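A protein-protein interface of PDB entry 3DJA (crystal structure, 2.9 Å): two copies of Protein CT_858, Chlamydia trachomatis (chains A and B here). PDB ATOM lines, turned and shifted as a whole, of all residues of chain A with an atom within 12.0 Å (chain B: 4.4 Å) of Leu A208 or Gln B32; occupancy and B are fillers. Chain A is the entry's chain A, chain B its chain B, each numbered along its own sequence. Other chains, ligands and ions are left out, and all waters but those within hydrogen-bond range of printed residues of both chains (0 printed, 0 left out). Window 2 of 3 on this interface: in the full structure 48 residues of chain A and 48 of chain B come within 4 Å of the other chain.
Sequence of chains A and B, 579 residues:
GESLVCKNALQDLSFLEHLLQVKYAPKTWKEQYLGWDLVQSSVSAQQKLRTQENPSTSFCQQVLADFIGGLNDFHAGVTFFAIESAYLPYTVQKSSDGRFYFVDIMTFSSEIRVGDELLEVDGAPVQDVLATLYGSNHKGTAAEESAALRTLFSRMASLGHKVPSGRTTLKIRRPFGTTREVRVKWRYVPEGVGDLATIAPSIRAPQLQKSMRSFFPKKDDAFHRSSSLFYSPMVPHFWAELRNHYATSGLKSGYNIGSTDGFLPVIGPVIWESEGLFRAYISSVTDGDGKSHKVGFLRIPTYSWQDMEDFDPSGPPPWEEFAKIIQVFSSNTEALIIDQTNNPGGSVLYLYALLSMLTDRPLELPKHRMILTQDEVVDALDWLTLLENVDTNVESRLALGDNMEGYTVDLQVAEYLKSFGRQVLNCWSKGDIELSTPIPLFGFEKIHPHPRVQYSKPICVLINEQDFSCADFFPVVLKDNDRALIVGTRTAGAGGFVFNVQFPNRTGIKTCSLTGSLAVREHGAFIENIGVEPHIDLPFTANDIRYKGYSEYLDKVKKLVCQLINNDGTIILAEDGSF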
ATOM      1  N   ARG A 204     -30.749  25.732 -24.743  1.00  0.00           N
ATOM      2  CA  ARG A 204     -30.280  25.529 -23.381  1.00  0.00           C
ATOM      3  C   ARG A 204     -29.136  26.487 -23.064  1.00  0.00           C
ATOM      4  O   ARG A 204     -28.510  27.035 -23.966  1.00  0.00           O
ATOM      5  CB  ARG A 204     -29.872  24.064 -23.146  1.00  0.00           C
ATOM      6  CG  ARG A 204     -31.042  23.169 -22.627  1.00  0.00           C
ATOM      7  CD  ARG A 204     -31.789  23.810 -21.413  1.00  0.00           C
ATOM      8  NE  ARG A 204     -30.900  24.147 -20.293  1.00  0.00           N
ATOM      9  CZ  ARG A 204     -31.186  25.032 -19.341  1.00  0.00           C
ATOM     10  NH1 ARG A 204     -32.342  25.684 -19.353  1.00  0.00           N
ATOM     11  NH2 ARG A 204     -30.309  25.272 -18.380  1.00  0.00           N
ATOM     12  N   ALA A 205     -28.897  26.721 -21.778  1.00  0.00           N
ATOM     13  CA  ALA A 205     -27.835  27.631 -21.359  1.00  0.00           C
ATOM     14  C   ALA A 205     -26.488  27.122 -21.852  1.00  0.00           C
ATOM     15  O   ALA A 205     -26.243  25.912 -21.899  1.00  0.00           O
ATOM     16  CB  ALA A 205     -27.823  27.762 -19.841  1.00  0.00           C
ATOM     17  N   PRO A 206     -25.587  28.036 -22.217  1.00  0.00           N
ATOM     18  CA  PRO A 206     -24.276  27.607 -22.702  1.00  0.00           C
ATOM     19  C   PRO A 206     -23.481  26.952 -21.595  1.00  0.00           C
ATOM     20  O   PRO A 206     -23.702  27.227 -20.420  1.00  0.00           O
ATOM     21  CB  PRO A 206     -23.643  28.911 -23.167  1.00  0.00           C
ATOM     22  CG  PRO A 206     -24.150  29.880 -22.140  1.00  0.00           C
ATOM     23  CD  PRO A 206     -25.625  29.497 -22.024  1.00  0.00           C
ATOM     24  N   GLN A 207     -22.566  26.073 -21.976  1.00  0.00           N
ATOM     25  CA  GLN A 207     -21.713  25.401 -21.012  1.00  0.00           C
ATOM     26  C   GLN A 207     -20.434  24.948 -21.686  1.00  0.00           C
ATOM     27  O   GLN A 207     -20.462  24.451 -22.808  1.00  0.00           O
ATOM     28  CB  GLN A 207     -22.423  24.202 -20.396  1.00  0.00           C
ATOM     29  CG  GLN A 207     -22.980  23.237 -21.406  1.00  0.00           C
ATOM     30  CD  GLN A 207     -23.425  21.934 -20.761  1.00  0.00           C
ATOM     31  OE1 GLN A 207     -24.217  21.933 -19.810  1.00  0.00           O
ATOM     32  NE2 GLN A 207     -22.916  20.814 -21.274  1.00  0.00           N
ATOM     33  N   LEU A 208     -19.309  25.141 -21.004  1.00  0.00           N
ATOM     34  CA  LEU A 208     -18.028  24.729 -21.549  1.00  0.00           C
ATOM     35  C   LEU A 208     -18.000  23.217 -21.638  1.00  0.00           C
ATOM     36  O   LEU A 208     -18.851  22.532 -21.058  1.00  0.00           O
ATOM     37  CB  LEU A 208     -16.878  25.178 -20.655  1.00  0.00           C
ATOM     38  CG  LEU A 208     -16.673  26.663 -20.406  1.00  0.00           C
ATOM     39  CD1 LEU A 208     -15.317  26.840 -19.753  1.00  0.00           C
ATOM     40  CD2 LEU A 208     -16.733  27.439 -21.713  1.00  0.00           C
ATOM     41  N   GLN A 209     -17.007  22.708 -22.362  1.00  0.00           N
ATOM     42  CA  GLN A 209     -16.818  21.271 -22.540  1.00  0.00           C
ATOM     43  C   GLN A 209     -18.172  20.552 -22.640  1.00  0.00           C
ATOM     44  O   GLN A 209     -18.288  19.476 -23.234  1.00  0.00           O
ATOM     45  CB  GLN A 209     -16.010  20.699 -21.360  1.00  0.00           C
ATOM     46  CG  GLN A 209     -14.969  21.652 -20.741  1.00  0.00           C
ATOM     47  CD  GLN A 209     -13.840  22.049 -21.691  1.00  0.00           C
ATOM     48  OE1 GLN A 209     -12.937  22.803 -21.314  1.00  0.00           O
ATOM     49  NE2 GLN A 209     -13.888  21.546 -22.923  1.00  0.00           N
ATOM     50  N   THR B  28     -19.275  32.504 -20.930  1.00  0.00           N
ATOM     51  CA  THR B  28     -19.269  31.282 -20.141  1.00  0.00           C
ATOM     52  C   THR B  28     -17.883  30.897 -19.655  1.00  0.00           C
ATOM     53  O   THR B  28     -17.745  30.276 -18.609  1.00  0.00           O
ATOM     54  CB  THR B  28     -19.802  30.098 -20.948  1.00  0.00           C
ATOM     55  OG1 THR B  28     -20.760  30.560 -21.911  1.00  0.00           O
ATOM     56  CG2 THR B  28     -20.448  29.084 -20.017  1.00  0.00           C
ATOM     57  N   TRP B  29     -16.859  31.243 -20.431  1.00  0.00           N
ATOM     58  CA  TRP B  29     -15.488  30.909 -20.067  1.00  0.00           C
ATOM     59  C   TRP B  29     -15.011  31.802 -18.950  1.00  0.00           C
ATOM     60  O   TRP B  29     -14.593  31.314 -17.906  1.00  0.00           O
ATOM     61  CB  TRP B  29     -14.557  31.039 -21.281  1.00  0.00           C
ATOM     62  CG  TRP B  29     -13.071  31.134 -20.950  1.00  0.00           C
ATOM     63  CD1 TRP B  29     -12.290  32.259 -20.999  1.00  0.00           C
ATOM     64  CD2 TRP B  29     -12.210  30.075 -20.504  1.00  0.00           C
ATOM     65  NE1 TRP B  29     -11.002  31.969 -20.613  1.00  0.00           N
ATOM     66  CE2 TRP B  29     -10.924  30.640 -20.299  1.00  0.00           C
ATOM     67  CE3 TRP B  29     -12.400  28.706 -20.253  1.00  0.00           C
ATOM     68  CZ2 TRP B  29      -9.834  29.886 -19.856  1.00  0.00           C
ATOM     69  CZ3 TRP B  29     -11.313  27.952 -19.809  1.00  0.00           C
ATOM     70  CH2 TRP B  29     -10.044  28.551 -19.613  1.00  0.00           C
ATOM     71  N   LYS B  30     -15.080  33.112 -19.168  1.00  0.00           N
ATOM     72  CA  LYS B  30     -14.638  34.080 -18.165  1.00  0.00           C
ATOM     73  C   LYS B  30     -15.324  33.875 -16.814  1.00  0.00           C
ATOM     74  O   LYS B  30     -14.812  34.299 -15.779  1.00  0.00           O
ATOM     75  CB  LYS B  30     -14.912  35.501 -18.641  1.00  0.00           C
ATOM     76  CG  LYS B  30     -14.345  35.809 -19.990  1.00  0.00           C
ATOM     77  CD  LYS B  30     -12.836  35.874 -20.001  1.00  0.00           C
ATOM     78  CE  LYS B  30     -12.380  36.208 -21.416  1.00  0.00           C
ATOM     79  NZ  LYS B  30     -10.909  36.204 -21.665  1.00  0.00           N
ATOM     80  N   GLU B  31     -16.489  33.243 -16.819  1.00  0.00           N
ATOM     81  CA  GLU B  31     -17.182  33.012 -15.569  1.00  0.00           C
ATOM     82  C   GLU B  31     -16.467  31.920 -14.785  1.00  0.00           C
ATOM     83  O   GLU B  31     -16.143  32.103 -13.611  1.00  0.00           O
ATOM     84  CB  GLU B  31     -18.629  32.612 -15.834  1.00  0.00           C
ATOM     85  CG  GLU B  31     -19.395  33.653 -16.612  1.00  0.00           C
ATOM     86  CD  GLU B  31     -20.877  33.370 -16.658  1.00  0.00           C
ATOM     87  OE1 GLU B  31     -21.257  32.221 -16.972  1.00  0.00           O
ATOM     88  OE2 GLU B  31     -21.667  34.300 -16.387  1.00  0.00           O
ATOM     89  N   GLN B  32     -16.205  30.795 -15.447  1.00  0.00           N
ATOM     90  CA  GLN B  32     -15.536  29.659 -14.824  1.00  0.00           C
ATOM     91  C   GLN B  32     -14.066  29.888 -14.529  1.00  0.00           C
ATOM     92  O   GLN B  32     -13.567  29.465 -13.494  1.00  0.00           O
ATOM     93  CB  GLN B  32     -15.666  28.433 -15.710  1.00  0.00           C
ATOM     94  CG  GLN B  32     -17.094  28.128 -16.094  1.00  0.00           C
ATOM     95  CD  GLN B  32     -17.410  26.652 -16.002  1.00  0.00           C
ATOM     96  OE1 GLN B  32     -17.388  26.066 -14.912  1.00  0.00           O
ATOM     97  NE2 GLN B  32     -17.698  26.033 -17.146  1.00  0.00           N
ATOM     98  N   TYR B  33     -13.373  30.552 -15.437  1.00  0.00           N
ATOM     99  CA  TYR B  33     -11.949  30.809 -15.265  1.00  0.00           C
ATOM    100  C   TYR B  33     -11.626  31.976 -14.334  1.00  0.00           C
ATOM    101  O   TYR B  33     -10.756  31.859 -13.484  1.00  0.00           O
ATOM    102  CB  TYR B  33     -11.309  31.037 -16.642  1.00  0.00           C
ATOM    103  CG  TYR B  33      -9.859  31.487 -16.631  1.00  0.00           C
ATOM    104  CD1 TYR B  33      -8.827  30.606 -16.298  1.00  0.00           C
ATOM    105  CD2 TYR B  33      -9.519  32.795 -16.990  1.00  0.00           C
ATOM    106  CE1 TYR B  33      -7.488  31.021 -16.330  1.00  0.00           C
ATOM    107  CE2 TYR B  33      -8.191  33.217 -17.027  1.00  0.00           C
ATOM    108  CZ  TYR B  33      -7.180  32.329 -16.698  1.00  0.00           C
ATOM    109  OH  TYR B  33      -5.870  32.752 -16.744  1.00  0.00           O
ATOM    110  N   LEU B  34     -12.323  33.097 -14.497  1.00  0.00           N
ATOM    111  CA  LEU B  34     -12.091  34.289 -13.681  1.00  0.00           C
ATOM    112  C   LEU B  34     -13.149  34.492 -12.600  1.00  0.00           C
ATOM    113  O   LEU B  34     -13.196  35.549 -11.967  1.00  0.00           O
ATOM    114  CB  LEU B  34     -12.089  35.530 -14.563  1.00  0.00           C
ATOM    115  CG  LEU B  34     -11.106  35.582 -15.720  1.00  0.00           C
ATOM    116  CD1 LEU B  34     -11.387  36.813 -16.564  1.00  0.00           C
ATOM    117  CD2 LEU B  34      -9.702  35.632 -15.177  1.00  0.00           C
ATOM    118  N   GLY B  35     -14.006  33.495 -12.410  1.00  0.00           N
ATOM    119  CA  GLY B  35     -15.053  33.606 -11.412  1.00  0.00           C
ATOM    120  C   GLY B  35     -15.847  34.888 -11.593  1.00  0.00           C
ATOM    121  O   GLY B  35     -16.515  35.360 -10.661  1.00  0.00           O
ATOM    122  N   LEU B 435     -23.384  29.194 -27.395  1.00  0.00           N
ATOM    123  CA  LEU B 435     -21.976  28.865 -27.555  1.00  0.00           C
ATOM    124  C   LEU B 435     -21.974  27.608 -28.418  1.00  0.00           C
ATOM    125  O   LEU B 435     -21.828  26.498 -27.906  1.00  0.00           O
ATOM    126  CB  LEU B 435     -21.358  28.575 -26.197  1.00  0.00           C
ATOM    127  CG  LEU B 435     -19.852  28.358 -26.145  1.00  0.00           C
ATOM    128  CD1 LEU B 435     -19.126  29.553 -26.730  1.00  0.00           C
ATOM    129  CD2 LEU B 435     -19.451  28.161 -24.704  1.00  0.00           C
ATOM    130  N   PHE B 526      -8.603  25.575 -24.872  1.00  0.00           N
ATOM    131  CA  PHE B 526      -8.926  26.862 -25.473  1.00  0.00           C
ATOM    132  C   PHE B 526      -7.680  27.684 -25.651  1.00  0.00           C
ATOM    133  O   PHE B 526      -6.589  27.257 -25.281  1.00  0.00           O
ATOM    134  CB  PHE B 526      -9.876  27.653 -24.594  1.00  0.00           C
ATOM    135  CG  PHE B 526     -11.184  26.996 -24.395  1.00  0.00           C
ATOM    136  CD1 PHE B 526     -11.525  26.469 -23.159  1.00  0.00           C
ATOM    137  CD2 PHE B 526     -12.081  26.891 -25.448  1.00  0.00           C
ATOM    138  CE1 PHE B 526     -12.752  25.841 -22.973  1.00  0.00           C
ATOM    139  CE2 PHE B 526     -13.312  26.264 -25.274  1.00  0.00           C
ATOM    140  CZ  PHE B 526     -13.650  25.739 -24.036  1.00  0.00           C
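Among the printed residues, pairs that only touch across the chains: Pro A206 with Thr B28 (3.5 Å), Pro A206 with Leu B435 (3.8 Å), Leu A208 with Trp B29 (3.5 Å), Leu A208 with Gln B32 (3.5 Å) and Gln A209 with Phe B526 (3.5 Å).
No position is printed for both chains. Of the 5 pairs that touch across the chains among the printed residues, none has its exchanged pair printed and touching as well.
Of the 10 printed residues of chain B, 5 touch a printed residue of chain A. Printed residues of chain B that touch a printed residue of chain A: Thr B28, Trp B29, Gln B32, Leu B435 and Phe B526. Of the 6 printed residues of chain A, 3 touch a printed residue of chain B. Printed residues of chain A that touch a printed residue of chain B: Pro A206, Leu A208 and Gln A209. Hydrophobic or aromatic side chains of chain A that line the printed part of chain B: Pro A206 and Leu A208. Among the printed residues, no Asp or Glu carboxylate lies within 4 Å of a Lys or Arg side-chain nitrogen of the other chain.
Arg A204 touches none of the printed residues of chain B. Leu A208 touches just these residues of chain B: Trp B29 and Gln B32. Printed residues of chain B within 4 Å of Gln A209: Phe B526 (3.5 Å). Of the printed residues of chain A, Thr B28 touches Pro A206. Trp B29 touches one residue of chain A. No residue of chain A comes within 4 Å of Glu B31. Printed residues of chain A within 4 Å of Gln B32: Leu A208 (3.5 Å). Of the printed residues of chain A, Phe B526 touches Gln A209. The nearest printed residue of chain B that does not touch Leu A208 is Leu B435 (4.1 Å). The nearest residue of chain A that does not touch Gln B32 is Gln A207 (5.4 Å).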
